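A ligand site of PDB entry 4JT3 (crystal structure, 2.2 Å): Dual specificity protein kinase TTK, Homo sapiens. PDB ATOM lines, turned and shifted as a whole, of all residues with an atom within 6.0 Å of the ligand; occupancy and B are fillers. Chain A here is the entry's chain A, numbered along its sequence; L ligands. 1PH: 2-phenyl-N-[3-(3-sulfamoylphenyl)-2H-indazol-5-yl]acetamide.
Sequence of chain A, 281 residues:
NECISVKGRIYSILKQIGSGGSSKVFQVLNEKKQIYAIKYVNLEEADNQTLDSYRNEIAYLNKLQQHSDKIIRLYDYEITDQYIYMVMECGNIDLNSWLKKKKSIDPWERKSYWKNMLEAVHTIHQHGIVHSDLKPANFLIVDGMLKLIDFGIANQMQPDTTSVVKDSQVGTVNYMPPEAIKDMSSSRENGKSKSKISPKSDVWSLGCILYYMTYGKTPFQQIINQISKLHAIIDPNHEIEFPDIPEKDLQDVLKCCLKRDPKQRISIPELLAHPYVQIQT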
ATOM      1  N   LYS A  15      34.121 -17.916  -2.926  1.00  0.00           N
ATOM      2  CA  LYS A  15      32.830 -17.617  -2.303  1.00  0.00           C
ATOM      3  C   LYS A  15      31.679 -18.104  -3.213  1.00  0.00           C
ATOM      4  O   LYS A  15      31.842 -18.141  -4.432  1.00  0.00           O
ATOM      5  CB  LYS A  15      32.731 -16.087  -2.004  1.00  0.00           C
ATOM      6  CG  LYS A  15      31.364 -15.419  -2.183  1.00  0.00           C
ATOM      7  CD  LYS A  15      31.002 -14.500  -1.035  1.00  0.00           C
ATOM      8  CE  LYS A  15      29.624 -13.907  -1.218  1.00  0.00           C
ATOM      9  NZ  LYS A  15      29.195 -13.120  -0.041  1.00  0.00           N
ATOM     10  N   ILE A  17      28.271 -17.418  -4.986  1.00  0.00           N
ATOM     11  CA  ILE A  17      27.480 -16.293  -5.507  1.00  0.00           C
ATOM     12  C   ILE A  17      25.991 -16.540  -5.205  1.00  0.00           C
ATOM     13  O   ILE A  17      25.348 -15.675  -4.605  1.00  0.00           O
ATOM     14  CB  ILE A  17      27.761 -16.074  -7.027  1.00  0.00           C
ATOM     15  CG1 ILE A  17      29.214 -15.606  -7.276  1.00  0.00           C
ATOM     16  CG2 ILE A  17      26.750 -15.090  -7.649  1.00  0.00           C
ATOM     17  CD1 ILE A  17      29.773 -15.934  -8.667  1.00  0.00           C
ATOM     18  N   GLY A  18      25.479 -17.694  -5.630  1.00  0.00           N
ATOM     19  CA  GLY A  18      24.087 -18.067  -5.431  1.00  0.00           C
ATOM     20  C   GLY A  18      23.816 -19.557  -5.567  1.00  0.00           C
ATOM     21  O   GLY A  18      24.688 -20.318  -6.011  1.00  0.00           O
ATOM     22  N   SER A  19      22.602 -19.970  -5.190  1.00  0.00           N
ATOM     23  CA  SER A  19      22.123 -21.347  -5.240  1.00  0.00           C
ATOM     24  C   SER A  19      20.637 -21.372  -5.581  1.00  0.00           C
ATOM     25  O   SER A  19      19.886 -20.519  -5.102  1.00  0.00           O
ATOM     26  CB  SER A  19      22.376 -22.063  -3.921  1.00  0.00           C
ATOM     27  OG  SER A  19      21.715 -21.436  -2.841  1.00  0.00           O
ATOM     28  N   GLY A  20      20.224 -22.348  -6.393  1.00  0.00           N
ATOM     29  CA  GLY A  20      18.833 -22.471  -6.807  1.00  0.00           C
ATOM     30  C   GLY A  20      18.487 -23.703  -7.618  1.00  0.00           C
ATOM     31  O   GLY A  20      18.887 -23.800  -8.782  1.00  0.00           O
ATOM     32  N   SER A  23      21.253 -26.364  -8.606  1.00  0.00           N
ATOM     33  CA  SER A  23      22.306 -25.536  -9.203  1.00  0.00           C
ATOM     34  C   SER A  23      22.927 -24.570  -8.192  1.00  0.00           C
ATOM     35  O   SER A  23      22.239 -24.080  -7.288  1.00  0.00           O
ATOM     36  CB  SER A  23      21.772 -24.753 -10.394  1.00  0.00           C
ATOM     37  OG  SER A  23      21.416 -25.622 -11.463  1.00  0.00           O
ATOM     38  N   LYS A  24      24.204 -24.257  -8.388  1.00  0.00           N
ATOM     39  CA  LYS A  24      24.991 -23.334  -7.571  1.00  0.00           C
ATOM     40  C   LYS A  24      25.986 -22.574  -8.422  1.00  0.00           C
ATOM     41  O   LYS A  24      26.537 -23.101  -9.343  1.00  0.00           O
ATOM     42  CB  LYS A  24      25.803 -24.103  -6.547  1.00  0.00           C
ATOM     43  CG  LYS A  24      25.078 -24.600  -5.328  1.00  0.00           C
ATOM     44  CD  LYS A  24      26.036 -25.342  -4.432  1.00  0.00           C
ATOM     45  CE  LYS A  24      25.294 -26.109  -3.351  1.00  0.00           C
ATOM     46  NZ  LYS A  24      26.199 -27.075  -2.672  1.00  0.00           N
ATOM     47  N   VAL A  25      26.244 -21.324  -8.066  1.00  0.00           N
ATOM     48  CA  VAL A  25      27.213 -20.483  -8.773  1.00  0.00           C
ATOM     49  C   VAL A  25      28.247 -20.023  -7.745  1.00  0.00           C
ATOM     50  O   VAL A  25      27.880 -19.552  -6.669  1.00  0.00           O
ATOM     51  CB  VAL A  25      26.559 -19.292  -9.532  1.00  0.00           C
ATOM     52  CG1 VAL A  25      27.591 -18.549 -10.379  1.00  0.00           C
ATOM     53  CG2 VAL A  25      25.408 -19.750 -10.413  1.00  0.00           C
ATOM     54  N   GLN A  27      32.337 -18.109  -7.052  1.00  0.00           N
ATOM     55  CA  GLN A  27      33.490 -17.299  -7.447  1.00  0.00           C
ATOM     56  C   GLN A  27      34.678 -18.231  -7.304  1.00  0.00           C
ATOM     57  O   GLN A  27      34.833 -18.854  -6.253  1.00  0.00           O
ATOM     58  CB  GLN A  27      33.632 -16.081  -6.522  1.00  0.00           C
ATOM     59  CG  GLN A  27      32.936 -14.817  -6.981  1.00  0.00           C
ATOM     60  CD  GLN A  27      33.398 -13.614  -6.192  1.00  0.00           C
ATOM     61  OE1 GLN A  27      33.776 -13.703  -5.013  1.00  0.00           O
ATOM     62  NE2 GLN A  27      33.375 -12.456  -6.805  1.00  0.00           N
ATOM     63  N   ILE A  35      40.094 -14.526 -11.642  1.00  0.00           N
ATOM     64  CA  ILE A  35      38.722 -14.871 -11.276  1.00  0.00           C
ATOM     65  C   ILE A  35      37.880 -15.377 -12.479  1.00  0.00           C
ATOM     66  O   ILE A  35      38.059 -14.941 -13.615  1.00  0.00           O
ATOM     67  CB  ILE A  35      37.989 -13.732 -10.499  1.00  0.00           C
ATOM     68  CG1 ILE A  35      36.834 -14.306  -9.648  1.00  0.00           C
ATOM     69  CG2 ILE A  35      37.531 -12.600 -11.443  1.00  0.00           C
ATOM     70  CD1 ILE A  35      36.281 -13.459  -8.556  1.00  0.00           C
ATOM     71  N   ALA A  37      33.631 -17.543 -12.879  1.00  0.00           N
ATOM     72  CA  ALA A  37      32.412 -17.953 -12.204  1.00  0.00           C
ATOM     73  C   ALA A  37      32.045 -19.340 -12.679  1.00  0.00           C
ATOM     74  O   ALA A  37      31.837 -19.546 -13.878  1.00  0.00           O
ATOM     75  CB  ALA A  37      31.282 -16.963 -12.486  1.00  0.00           C
ATOM     76  N   LYS A  39      29.450 -22.467 -12.622  1.00  0.00           N
ATOM     77  CA  LYS A  39      28.103 -22.933 -12.322  1.00  0.00           C
ATOM     78  C   LYS A  39      28.160 -24.445 -12.188  1.00  0.00           C
ATOM     79  O   LYS A  39      28.669 -25.125 -13.089  1.00  0.00           O
ATOM     80  CB  LYS A  39      27.079 -22.485 -13.389  1.00  0.00           C
ATOM     81  CG  LYS A  39      25.722 -23.209 -13.327  1.00  0.00           C
ATOM     82  CD  LYS A  39      24.535 -22.267 -13.255  1.00  0.00           C
ATOM     83  CE  LYS A  39      23.659 -22.363 -14.473  1.00  0.00           C
ATOM     84  NZ  LYS A  39      22.279 -21.862 -14.213  1.00  0.00           N
ATOM     85  N   ILE A  72      27.018 -13.907 -22.152  1.00  0.00           N
ATOM     86  CA  ILE A  72      28.048 -14.322 -21.190  1.00  0.00           C
ATOM     87  C   ILE A  72      29.117 -15.209 -21.874  1.00  0.00           C
ATOM     88  O   ILE A  72      28.769 -16.075 -22.681  1.00  0.00           O
ATOM     89  CB  ILE A  72      27.440 -15.015 -19.924  1.00  0.00           C
ATOM     90  CG1 ILE A  72      28.499 -15.297 -18.836  1.00  0.00           C
ATOM     91  CG2 ILE A  72      26.647 -16.280 -20.261  1.00  0.00           C
ATOM     92  CD1 ILE A  72      28.529 -14.323 -17.748  1.00  0.00           C
ATOM     93  N   MET A  88      32.682 -19.791 -16.541  1.00  0.00           N
ATOM     94  CA  MET A  88      32.222 -18.562 -17.184  1.00  0.00           C
ATOM     95  C   MET A  88      32.922 -17.312 -16.660  1.00  0.00           C
ATOM     96  O   MET A  88      33.647 -17.353 -15.658  1.00  0.00           O
ATOM     97  CB  MET A  88      30.712 -18.391 -16.986  1.00  0.00           C
ATOM     98  CG  MET A  88      29.873 -19.409 -17.719  1.00  0.00           C
ATOM     99  SD  MET A  88      28.123 -19.276 -17.297  1.00  0.00           S
ATOM    100  CE  MET A  88      28.150 -19.927 -15.658  1.00  0.00           C
ATOM    101  N   GLU A  89      32.671 -16.195 -17.350  1.00  0.00           N
ATOM    102  CA  GLU A  89      33.133 -14.847 -17.034  1.00  0.00           C
ATOM    103  C   GLU A  89      32.473 -14.414 -15.721  1.00  0.00           C
ATOM    104  O   GLU A  89      31.291 -14.686 -15.517  1.00  0.00           O
ATOM    105  CB  GLU A  89      32.721 -13.930 -18.193  1.00  0.00           C
ATOM    106  CG  GLU A  89      33.373 -12.563 -18.225  1.00  0.00           C
ATOM    107  CD  GLU A  89      33.030 -11.747 -19.462  1.00  0.00           C
ATOM    108  OE1 GLU A  89      31.893 -11.876 -19.967  1.00  0.00           O
ATOM    109  OE2 GLU A  89      33.900 -10.964 -19.911  1.00  0.00           O
ATOM    110  N   CYS A  90      33.246 -13.781 -14.820  1.00  0.00           N
ATOM    111  CA  CYS A  90      32.692 -13.322 -13.554  1.00  0.00           C
ATOM    112  C   CYS A  90      32.227 -11.868 -13.707  1.00  0.00           C
ATOM    113  O   CYS A  90      32.983 -11.035 -14.207  1.00  0.00           O
ATOM    114  CB  CYS A  90      33.682 -13.479 -12.410  1.00  0.00           C
ATOM    115  SG  CYS A  90      32.931 -13.384 -10.761  1.00  0.00           S
ATOM    116  N   GLY A  91      30.990 -11.606 -13.302  1.00  0.00           N
ATOM    117  CA  GLY A  91      30.365 -10.299 -13.379  1.00  0.00           C
ATOM    118  C   GLY A  91      30.350  -9.535 -12.070  1.00  0.00           C
ATOM    119  O   GLY A  91      30.906 -10.000 -11.081  1.00  0.00           O
ATOM    120  N   ASN A  92      29.687  -8.365 -12.071  1.00  0.00           N
ATOM    121  CA  ASN A  92      29.587  -7.484 -10.908  1.00  0.00           C
ATOM    122  C   ASN A  92      28.311  -7.768 -10.107  1.00  0.00           C
ATOM    123  O   ASN A  92      28.395  -7.974  -8.893  1.00  0.00           O
ATOM    124  CB  ASN A  92      29.623  -6.005 -11.328  1.00  0.00           C
ATOM    125  CG  ASN A  92      30.897  -5.598 -12.029  1.00  0.00           C
ATOM    126  OD1 ASN A  92      31.884  -5.219 -11.412  1.00  0.00           O
ATOM    127  ND2 ASN A  92      30.877  -5.649 -13.354  1.00  0.00           N
ATOM    128  N   ILE A  93      27.144  -7.738 -10.774  1.00  0.00           N
ATOM    129  CA  ILE A  93      25.817  -7.937 -10.170  1.00  0.00           C
ATOM    130  C   ILE A  93      24.772  -8.219 -11.265  1.00  0.00           C
ATOM    131  O   ILE A  93      24.923  -7.751 -12.393  1.00  0.00           O
ATOM    132  CB  ILE A  93      25.437  -6.673  -9.308  1.00  0.00           C
ATOM    133  CG1 ILE A  93      24.191  -6.908  -8.418  1.00  0.00           C
ATOM    134  CG2 ILE A  93      25.347  -5.378 -10.150  1.00  0.00           C
ATOM    135  CD1 ILE A  93      24.068  -5.978  -7.190  1.00  0.00           C
ATOM    136  N   ASP A  94      23.714  -8.983 -10.917  1.00  0.00           N
ATOM    137  CA  ASP A  94      22.617  -9.241 -11.842  1.00  0.00           C
ATOM    138  C   ASP A  94      21.742  -7.979 -11.902  1.00  0.00           C
ATOM    139  O   ASP A  94      21.724  -7.211 -10.938  1.00  0.00           O
ATOM    140  CB  ASP A  94      21.808 -10.486 -11.419  1.00  0.00           C
ATOM    141  CG  ASP A  94      21.147 -10.386 -10.067  1.00  0.00           C
ATOM    142  OD1 ASP A  94      21.852 -10.526  -9.042  1.00  0.00           O
ATOM    143  OD2 ASP A  94      19.911 -10.187 -10.026  1.00  0.00           O
ATOM    144  N   LEU A 140      23.207  -9.742 -16.730  1.00  0.00           N
ATOM    145  CA  LEU A 140      24.317  -9.517 -15.815  1.00  0.00           C
ATOM    146  C   LEU A 140      25.179  -8.326 -16.259  1.00  0.00           C
ATOM    147  O   LEU A 140      25.520  -8.223 -17.437  1.00  0.00           O
ATOM    148  CB  LEU A 140      25.177 -10.796 -15.739  1.00  0.00           C
ATOM    149  CG  LEU A 140      26.473 -10.730 -14.917  1.00  0.00           C
ATOM    150  CD1 LEU A 140      26.179 -10.732 -13.437  1.00  0.00           C
ATOM    151  CD2 LEU A 140      27.380 -11.880 -15.239  1.00  0.00           C
ATOM    152  N   ILE A 149      22.584 -14.109 -19.576  1.00  0.00           N
ATOM    153  CA  ILE A 149      23.193 -15.302 -18.990  1.00  0.00           C
ATOM    154  C   ILE A 149      22.501 -16.602 -19.438  1.00  0.00           C
ATOM    155  O   ILE A 149      23.204 -17.588 -19.644  1.00  0.00           O
ATOM    156  CB  ILE A 149      23.334 -15.248 -17.433  1.00  0.00           C
ATOM    157  CG1 ILE A 149      21.985 -14.947 -16.718  1.00  0.00           C
ATOM    158  CG2 ILE A 149      24.433 -14.273 -17.025  1.00  0.00           C
ATOM    159  CD1 ILE A 149      21.900 -15.404 -15.244  1.00  0.00           C
ATOM    160  N   ASP A 150      21.167 -16.609 -19.613  1.00  0.00           N
ATOM    161  CA  ASP A 150      20.421 -17.791 -20.037  1.00  0.00           C
ATOM    162  C   ASP A 150      19.403 -17.459 -21.146  1.00  0.00           C
ATOM    163  O   ASP A 150      18.993 -16.306 -21.273  1.00  0.00           O
ATOM    164  CB  ASP A 150      19.721 -18.459 -18.841  1.00  0.00           C
ATOM    165  CG  ASP A 150      18.683 -17.591 -18.161  1.00  0.00           C
ATOM    166  OD1 ASP A 150      19.075 -16.715 -17.363  1.00  0.00           O
ATOM    167  OD2 ASP A 150      17.481 -17.793 -18.428  1.00  0.00           O
HETATM  168  C10 1PH L   1      27.961 -13.898 -12.082  1.00  0.00           C
HETATM  169  N11 1PH L   1      29.114 -13.847 -12.790  1.00  0.00           N
HETATM  170  N12 1PH L   1      29.078 -14.750 -13.810  1.00  0.00           N
HETATM  171  C13 1PH L   1      27.889 -15.437 -13.740  1.00  0.00           C
HETATM  172  C14 1PH L   1      27.353 -16.492 -14.539  1.00  0.00           C
HETATM  173  C15 1PH L   1      26.087 -16.999 -14.257  1.00  0.00           C
HETATM  174  C16 1PH L   1      25.340 -16.493 -13.176  1.00  0.00           C
HETATM  175  C18 1PH L   1      23.328 -18.137 -13.271  1.00  0.00           C
HETATM  176  C22 1PH L   1      21.902 -18.198 -10.211  1.00  0.00           C
HETATM  177  C20 1PH L   1      21.967 -18.422 -12.703  1.00  0.00           C
HETATM  178  C21 1PH L   1      21.924 -19.023 -11.338  1.00  0.00           C
HETATM  179  C23 1PH L   1      21.854 -18.761  -8.933  1.00  0.00           C
HETATM  180  N01 1PH L   1      30.278  -9.853  -8.349  1.00  0.00           N
HETATM  181  S02 1PH L   1      29.800 -11.361  -7.984  1.00  0.00           S
HETATM  182  O03 1PH L   1      29.408 -11.484  -6.609  1.00  0.00           O
HETATM  183  O04 1PH L   1      30.921 -12.270  -8.069  1.00  0.00           O
HETATM  184  C05 1PH L   1      28.466 -11.881  -9.031  1.00  0.00           C
HETATM  185  C06 1PH L   1      27.158 -11.515  -8.714  1.00  0.00           C
HETATM  186  C07 1PH L   1      26.106 -11.935  -9.526  1.00  0.00           C
HETATM  187  C08 1PH L   1      26.368 -12.728 -10.645  1.00  0.00           C
HETATM  188  C09 1PH L   1      27.671 -13.108 -10.967  1.00  0.00           C
HETATM  189  N17 1PH L   1      24.024 -16.964 -12.794  1.00  0.00           N
HETATM  190  O19 1PH L   1      23.794 -18.913 -14.094  1.00  0.00           O
HETATM  191  C24 1PH L   1      21.822 -20.152  -8.789  1.00  0.00           C
HETATM  192  C25 1PH L   1      21.844 -20.977  -9.916  1.00  0.00           C
HETATM  193  C26 1PH L   1      21.884 -20.413 -11.189  1.00  0.00           C
HETATM  194  C27 1PH L   1      25.880 -15.471 -12.382  1.00  0.00           C
HETATM  195  C28 1PH L   1      27.167 -14.934 -12.675  1.00  0.00           C
HETATM  196  C29 1PH L   1      28.728 -12.675 -10.150  1.00  0.00           C
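N01 of the ligand is in hydrogen-bond range of O of Asn 92. O04 of the ligand is in hydrogen-bond range of NE2 of Gln 27 (2.8 Å). O of Glu 89 sits close to N12 of the ligand, 2.8 Å away. N of Gly 91 lies close to N11 of the ligand. A nitrogen (N01) of the ligand is in hydrogen-bond range of the backbone carbonyl oxygen of Gly 91 (2.8 Å). The side-chain amino group of Lys 39 sits at hydrogen-bond distance from an oxygen (O19) of the ligand (3.3 Å). An oxygen (O04) of the ligand is in hydrogen-bond range of the side-chain sulfur (SG) of Cys 90 (3.5 Å).
The backbone NH (N) of Gln 27 sits at hydrogen-bond distance from the backbone carbonyl oxygen (O) of Lys 15, at 2.7 Å. The backbone carbonyl oxygen (O) of Met 88 lies within hydrogen-bond range of the backbone NH (N) of Ala 37 (2.8 Å). O of Val 25 sits at hydrogen-bond distance from N of Ile 17. The backbone NH (N) of Val 25 is in hydrogen-bond range of the backbone carbonyl oxygen (O) of Gly 18 (2.8 Å).
Ile 17 touches the ligand (CG2 to C07, 3.7 Å). Gly 18 touches the ligand (C to C24, 3.8 Å). C of Ser 19 touches C24 of the ligand (3.6 Å). N of Gly 20 touches C24 of the ligand, 3.6 Å away. Ser 23 touches the ligand. Val 25 touches the ligand (CG2 to C26, 3.7 Å). Ala 37 touches the ligand (CB to N12, 3.4 Å). Ile 72 touches the ligand (CD1 to N12, 3.999 Å). Met 88 touches the ligand. CD1 of Leu 140 touches C08 of the ligand, 3.4 Å away. Ile 149 touches the ligand (CD1 to N17, 3.6 Å). Of the 23 residues printed, 17 come within 4 Å of the ligand. The nearest printed residue that does not touch the ligand is Asp 94 (4.05 Å).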
